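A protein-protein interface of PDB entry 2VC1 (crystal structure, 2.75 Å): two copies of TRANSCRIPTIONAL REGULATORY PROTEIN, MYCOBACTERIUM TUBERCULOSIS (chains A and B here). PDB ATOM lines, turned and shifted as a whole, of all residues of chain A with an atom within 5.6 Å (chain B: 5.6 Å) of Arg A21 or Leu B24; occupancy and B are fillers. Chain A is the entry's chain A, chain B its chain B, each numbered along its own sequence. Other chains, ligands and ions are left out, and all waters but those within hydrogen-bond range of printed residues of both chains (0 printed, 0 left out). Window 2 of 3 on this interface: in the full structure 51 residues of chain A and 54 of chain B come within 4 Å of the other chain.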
ATOM      1  N   ASP A  19       3.854  30.338  -4.212  1.00  0.00           N
ATOM      2  CA  ASP A  19       5.150  29.719  -4.134  1.00  0.00           C
ATOM      3  C   ASP A  19       6.194  30.309  -5.069  1.00  0.00           C
ATOM      4  O   ASP A  19       6.187  30.002  -6.236  1.00  0.00           O
ATOM      5  CB  ASP A  19       4.968  28.232  -4.412  1.00  0.00           C
ATOM      6  CG  ASP A  19       6.287  27.463  -4.368  1.00  0.00           C
ATOM      7  OD1 ASP A  19       7.408  28.013  -4.089  1.00  0.00           O
ATOM      8  OD2 ASP A  19       6.171  26.257  -4.617  1.00  0.00           O
ATOM      9  N   GLY A  20       7.128  31.097  -4.570  1.00  0.00           N
ATOM     10  CA  GLY A  20       7.953  31.889  -5.440  1.00  0.00           C
ATOM     11  C   GLY A  20       9.184  31.202  -5.927  1.00  0.00           C
ATOM     12  O   GLY A  20       9.858  31.717  -6.782  1.00  0.00           O
ATOM     13  N   ARG A  21       9.510  30.052  -5.343  1.00  0.00           N
ATOM     14  CA  ARG A  21      10.682  29.233  -5.717  1.00  0.00           C
ATOM     15  C   ARG A  21      10.154  28.206  -6.675  1.00  0.00           C
ATOM     16  O   ARG A  21      10.872  27.344  -7.110  1.00  0.00           O
ATOM     17  CB  ARG A  21      11.275  28.480  -4.494  1.00  0.00           C
ATOM     18  CG  ARG A  21      12.514  29.094  -3.854  1.00  0.00           C
ATOM     19  CD  ARG A  21      13.454  28.067  -3.170  1.00  0.00           C
ATOM     20  NE  ARG A  21      14.749  27.939  -3.875  1.00  0.00           N
ATOM     21  CZ  ARG A  21      15.542  28.966  -4.222  1.00  0.00           C
ATOM     22  NH1 ARG A  21      15.195  30.214  -3.946  1.00  0.00           N
ATOM     23  NH2 ARG A  21      16.697  28.754  -4.857  1.00  0.00           N
ATOM     24  N   ALA A  22       8.876  28.231  -6.974  1.00  0.00           N
ATOM     25  CA  ALA A  22       8.355  27.182  -7.836  1.00  0.00           C
ATOM     26  C   ALA A  22       8.973  27.181  -9.234  1.00  0.00           C
ATOM     27  O   ALA A  22       9.422  28.207  -9.767  1.00  0.00           O
ATOM     28  N   THR A  23       9.018  26.022  -9.848  1.00  0.00           N
ATOM     29  CA  THR A  23       9.833  25.971 -11.052  1.00  0.00           C
ATOM     30  C   THR A  23       9.034  25.926 -12.309  1.00  0.00           C
ATOM     31  O   THR A  23       7.859  25.539 -12.346  1.00  0.00           O
ATOM     32  CB  THR A  23      10.632  24.757 -11.052  1.00  0.00           C
ATOM     33  OG1 THR A  23       9.710  23.690 -10.701  1.00  0.00           O
ATOM     34  CG2 THR A  23      11.942  24.883 -10.003  1.00  0.00           C
ATOM     35  N   LEU B  16      18.635  35.294   0.331  1.00  0.00           N
ATOM     36  CA  LEU B  16      17.316  34.834   0.033  1.00  0.00           C
ATOM     37  C   LEU B  16      16.270  35.935   0.182  1.00  0.00           C
ATOM     38  O   LEU B  16      15.211  35.883  -0.463  1.00  0.00           O
ATOM     39  CB  LEU B  16      17.000  33.648   0.938  1.00  0.00           C
ATOM     40  CG  LEU B  16      17.504  32.307   0.411  1.00  0.00           C
ATOM     41  CD1 LEU B  16      16.816  31.130   1.151  1.00  0.00           C
ATOM     42  CD2 LEU B  16      17.212  32.276  -1.088  1.00  0.00           C
ATOM     43  N   ASP B  19      16.663  38.026  -2.958  1.00  0.00           N
ATOM     44  CA  ASP B  19      16.414  37.174  -4.147  1.00  0.00           C
ATOM     45  C   ASP B  19      15.842  35.834  -3.808  1.00  0.00           C
ATOM     46  O   ASP B  19      16.557  34.882  -3.583  1.00  0.00           O
ATOM     47  CB  ASP B  19      17.701  36.932  -4.947  1.00  0.00           C
ATOM     48  CG  ASP B  19      17.428  36.659  -6.419  1.00  0.00           C
ATOM     49  OD1 ASP B  19      16.260  36.296  -6.759  1.00  0.00           O
ATOM     50  OD2 ASP B  19      18.391  36.817  -7.226  1.00  0.00           O
ATOM     51  N   GLY B  20      14.540  35.751  -3.795  1.00  0.00           N
ATOM     52  CA  GLY B  20      13.908  34.493  -3.450  1.00  0.00           C
ATOM     53  C   GLY B  20      14.033  33.339  -4.436  1.00  0.00           C
ATOM     54  O   GLY B  20      13.750  32.199  -4.062  1.00  0.00           O
ATOM     55  N   ARG B  21      14.424  33.639  -5.684  1.00  0.00           N
ATOM     56  CA  ARG B  21      14.735  32.621  -6.702  1.00  0.00           C
ATOM     57  C   ARG B  21      16.228  32.405  -6.904  1.00  0.00           C
ATOM     58  O   ARG B  21      16.609  31.484  -7.630  1.00  0.00           O
ATOM     59  CB  ARG B  21      14.084  32.926  -8.057  1.00  0.00           C
ATOM     60  CG  ARG B  21      12.661  32.637  -8.051  1.00  0.00           C
ATOM     61  CD  ARG B  21      12.031  33.072  -9.284  1.00  0.00           C
ATOM     62  NE  ARG B  21      11.986  31.973 -10.256  1.00  0.00           N
ATOM     63  CZ  ARG B  21      11.124  30.959 -10.235  1.00  0.00           C
ATOM     64  NH1 ARG B  21      10.258  30.860  -9.274  1.00  0.00           N
ATOM     65  NH2 ARG B  21      11.149  30.020 -11.151  1.00  0.00           N
ATOM     66  N   ALA B  22      17.085  33.229  -6.293  1.00  0.00           N
ATOM     67  CA  ALA B  22      18.522  32.875  -6.183  1.00  0.00           C
ATOM     68  C   ALA B  22      18.642  31.358  -6.051  1.00  0.00           C
ATOM     69  O   ALA B  22      17.856  30.723  -5.318  1.00  0.00           O
ATOM     70  N   THR B  23      19.596  30.766  -6.763  1.00  0.00           N
ATOM     71  CA  THR B  23      19.615  29.299  -6.917  1.00  0.00           C
ATOM     72  C   THR B  23      20.584  28.567  -6.010  1.00  0.00           C
ATOM     73  O   THR B  23      21.672  29.099  -5.740  1.00  0.00           O
ATOM     74  CB  THR B  23      19.938  28.925  -8.339  1.00  0.00           C
ATOM     75  OG1 THR B  23      20.048  30.138  -9.116  1.00  0.00           O
ATOM     76  CG2 THR B  23      18.827  27.976  -8.897  1.00  0.00           C
ATOM     77  N   LEU B  24      20.202  27.352  -5.564  1.00  0.00           N
ATOM     78  CA  LEU B  24      20.975  26.647  -4.521  1.00  0.00           C
ATOM     79  C   LEU B  24      22.432  26.618  -5.030  1.00  0.00           C
ATOM     80  O   LEU B  24      23.389  26.745  -4.254  1.00  0.00           O
ATOM     81  CB  LEU B  24      20.404  25.257  -4.146  1.00  0.00           C
ATOM     82  CG  LEU B  24      18.926  24.914  -4.422  1.00  0.00           C
ATOM     83  CD1 LEU B  24      18.814  24.107  -5.735  1.00  0.00           C
ATOM     84  CD2 LEU B  24      18.207  24.122  -3.268  1.00  0.00           C
ATOM     85  N   SER B  25      22.562  26.520  -6.357  1.00  0.00           N
ATOM     86  CA  SER B  25      23.812  26.748  -7.116  1.00  0.00           C
ATOM     87  C   SER B  25      24.481  28.176  -6.876  1.00  0.00           C
ATOM     88  O   SER B  25      25.167  28.313  -5.869  1.00  0.00           O
ATOM     89  CB  SER B  25      23.570  26.316  -8.597  1.00  0.00           C
ATOM     90  OG  SER B  25      24.124  27.206  -9.551  1.00  0.00           O
ATOM     91  N   GLU B  26      24.272  29.194  -7.748  1.00  0.00           N
ATOM     92  CA  GLU B  26      24.760  30.621  -7.587  1.00  0.00           C
ATOM     93  C   GLU B  26      24.739  31.223  -6.151  1.00  0.00           C
ATOM     94  O   GLU B  26      25.484  32.190  -5.873  1.00  0.00           O
ATOM     95  CB  GLU B  26      24.094  31.621  -8.632  1.00  0.00           C
ATOM     96  N   LEU B  27      23.919  30.666  -5.243  1.00  0.00           N
ATOM     97  CA  LEU B  27      24.008  31.026  -3.810  1.00  0.00           C
ATOM     98  C   LEU B  27      25.415  30.727  -3.336  1.00  0.00           C
ATOM     99  O   LEU B  27      26.220  31.657  -3.244  1.00  0.00           O
ATOM    100  CB  LEU B  27      22.959  30.304  -2.934  1.00  0.00           C
ATOM    101  CG  LEU B  27      21.589  30.988  -2.696  1.00  0.00           C
ATOM    102  CD1 LEU B  27      20.718  30.250  -1.655  1.00  0.00           C
ATOM    103  CD2 LEU B  27      21.777  32.466  -2.298  1.00  0.00           C
ATOM    104  N   ALA B  28      25.688  29.430  -3.088  1.00  0.00           N
ATOM    105  CA  ALA B  28      27.045  28.823  -2.794  1.00  0.00           C
ATOM    106  C   ALA B  28      28.357  29.561  -3.175  1.00  0.00           C
ATOM    107  O   ALA B  28      29.308  29.549  -2.374  1.00  0.00           O
ATOM    108  CB  ALA B  28      27.110  27.321  -3.249  1.00  0.00           C
ATOM    109  N   VAL B  35      27.709  23.263  -3.058  1.00  0.00           N
ATOM    110  CA  VAL B  35      26.275  23.085  -3.502  1.00  0.00           C
ATOM    111  C   VAL B  35      25.362  22.229  -2.559  1.00  0.00           C
ATOM    112  O   VAL B  35      24.133  22.317  -2.580  1.00  0.00           O
ATOM    113  CB  VAL B  35      26.242  22.472  -4.961  1.00  0.00           C
ATOM    114  CG1 VAL B  35      25.251  23.306  -5.919  1.00  0.00           C
ATOM    115  CG2 VAL B  35      27.801  22.237  -5.556  1.00  0.00           C
ATOM    116  N   VAL B  38      25.210  24.132   1.093  1.00  0.00           N
ATOM    117  CA  VAL B  38      24.296  25.325   0.955  1.00  0.00           C
ATOM    118  C   VAL B  38      22.831  24.904   1.009  1.00  0.00           C
ATOM    119  O   VAL B  38      22.017  25.499   1.734  1.00  0.00           O
ATOM    120  CB  VAL B  38      24.559  26.172  -0.367  1.00  0.00           C
ATOM    121  CG1 VAL B  38      23.363  26.990  -0.767  1.00  0.00           C
ATOM    122  CG2 VAL B  38      25.727  27.095  -0.181  1.00  0.00           C
ATOM    123  N   GLN B  39      22.524  23.843   0.278  1.00  0.00           N
ATOM    124  CA  GLN B  39      21.180  23.362   0.168  1.00  0.00           C
ATOM    125  C   GLN B  39      20.643  22.781   1.460  1.00  0.00           C
ATOM    126  O   GLN B  39      19.432  22.590   1.663  1.00  0.00           O
ATOM    127  CB  GLN B  39      21.173  22.280  -0.877  1.00  0.00           C
ATOM    128  CG  GLN B  39      19.771  21.920  -1.350  1.00  0.00           C
ATOM    129  CD  GLN B  39      19.737  20.551  -1.962  1.00  0.00           C
ATOM    130  OE1 GLN B  39      18.719  19.855  -1.892  1.00  0.00           O
ATOM    131  NE2 GLN B  39      20.869  20.133  -2.554  1.00  0.00           N
ATOM    132  N   GLU B  46      14.316  26.332   7.040  1.00  0.00           N
ATOM    133  CA  GLU B  46      12.855  26.323   6.851  1.00  0.00           C
ATOM    134  C   GLU B  46      12.194  25.469   7.918  1.00  0.00           C
ATOM    135  O   GLU B  46      11.062  25.728   8.369  1.00  0.00           O
ATOM    136  CB  GLU B  46      12.458  25.799   5.458  1.00  0.00           C
ATOM    137  CG  GLU B  46      13.488  26.062   4.378  1.00  0.00           C
ATOM    138  CD  GLU B  46      13.013  25.732   2.992  1.00  0.00           C
ATOM    139  OE1 GLU B  46      12.175  24.802   2.863  1.00  0.00           O
ATOM    140  OE2 GLU B  46      13.498  26.402   2.039  1.00  0.00           O
ATOM    141  N   TYR B  54       8.255  31.405   0.430  1.00  0.00           N
ATOM    142  CA  TYR B  54       8.878  32.123  -0.696  1.00  0.00           C
ATOM    143  C   TYR B  54       7.778  32.840  -1.481  1.00  0.00           C
ATOM    144  O   TYR B  54       6.788  32.198  -1.799  1.00  0.00           O
ATOM    145  CB  TYR B  54       9.695  31.138  -1.582  1.00  0.00           C
ATOM    146  CG  TYR B  54      10.885  30.533  -0.839  1.00  0.00           C
ATOM    147  CD1 TYR B  54      10.767  29.282  -0.226  1.00  0.00           C
ATOM    148  CD2 TYR B  54      12.114  31.242  -0.717  1.00  0.00           C
ATOM    149  CE1 TYR B  54      11.818  28.732   0.517  1.00  0.00           C
ATOM    150  CE2 TYR B  54      13.193  30.698   0.010  1.00  0.00           C
ATOM    151  CZ  TYR B  54      13.026  29.429   0.640  1.00  0.00           C
ATOM    152  OH  TYR B  54      14.045  28.821   1.364  1.00  0.00           O
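The backbone carbonyl oxygen of Gly A20 is in hydrogen-bond range of the guanidinium group of Arg B21, 2.7 Å away. The backbone NH of Gly A20 sits at hydrogen-bond distance from the backbone carbonyl oxygen of Tyr B54, at 3.0 Å. The guanidinium group (NH1) of Arg A21 sits at hydrogen-bond distance from the backbone carbonyl oxygen (O) of Gly B20, 2.5 Å away. The guanidinium group (NH1) of Arg A21 is in hydrogen-bond range of the backbone carbonyl oxygen (O) of Ala B22, at 3.0 Å. The guanidinium group (NH1) of Arg B21 is in hydrogen-bond range of the backbone carbonyl oxygen (O) of Ala A22, at 2.8 Å.
OD1 of Asp A19 is in hydrogen-bond range of N of Arg A21, 3.2 Å away. OD1 of Asp A19 sits at hydrogen-bond distance from N of Ala A22 (3.2 Å). The side-chain carboxylate (OD1) of Asp B19 sits close to the backbone NH (N) of Arg B21. N of Ala B22 is in hydrogen-bond range of OD1 of Asp B19 (3.2 Å). OH of Tyr B54 lies within hydrogen-bond range of OE2 of Glu B46.
Asp A19 touches Tyr B54. Arg A21 touches Arg B21. Arg A21 touches Thr B23 (NH2 to CA, 3.6 Å). Arg A21 touches Leu B24. CG of Arg A21 touches CG of Tyr B54, 3.7 Å away.
Arg A21 touches six residues of chain B. Leu B24 touches just one residue of chain A: Arg A21. Printed residues of chain B within 4 Å of Gly A20: Arg B21 and Tyr B54. Of the printed residues of chain A, Arg B21 touches Gly A20, Arg A21 and Ala A22. The nearest printed residue of chain A that does not touch Leu B24 is Thr A23 (8.1 Å).
Hydrophobic or aromatic side chains of chain B within 4 Å of the printed part of chain A: Tyr B54. Among the printed residues, no Asp or Glu carboxylate lies within 4 Å of a Lys or Arg side-chain nitrogen of the other chain.
Gly A20 touches Arg B21, and with the chains exchanged Arg A21 touches Gly B20. Arg A21 touches its own counterpart, Arg B21. Arg A21 touches Ala B22, and with the chains exchanged Ala A22 touches Arg B21. Arg A21 touches Thr B23, but with the chains exchanged Thr A23 does not touch Arg B21 (4.3 Å).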
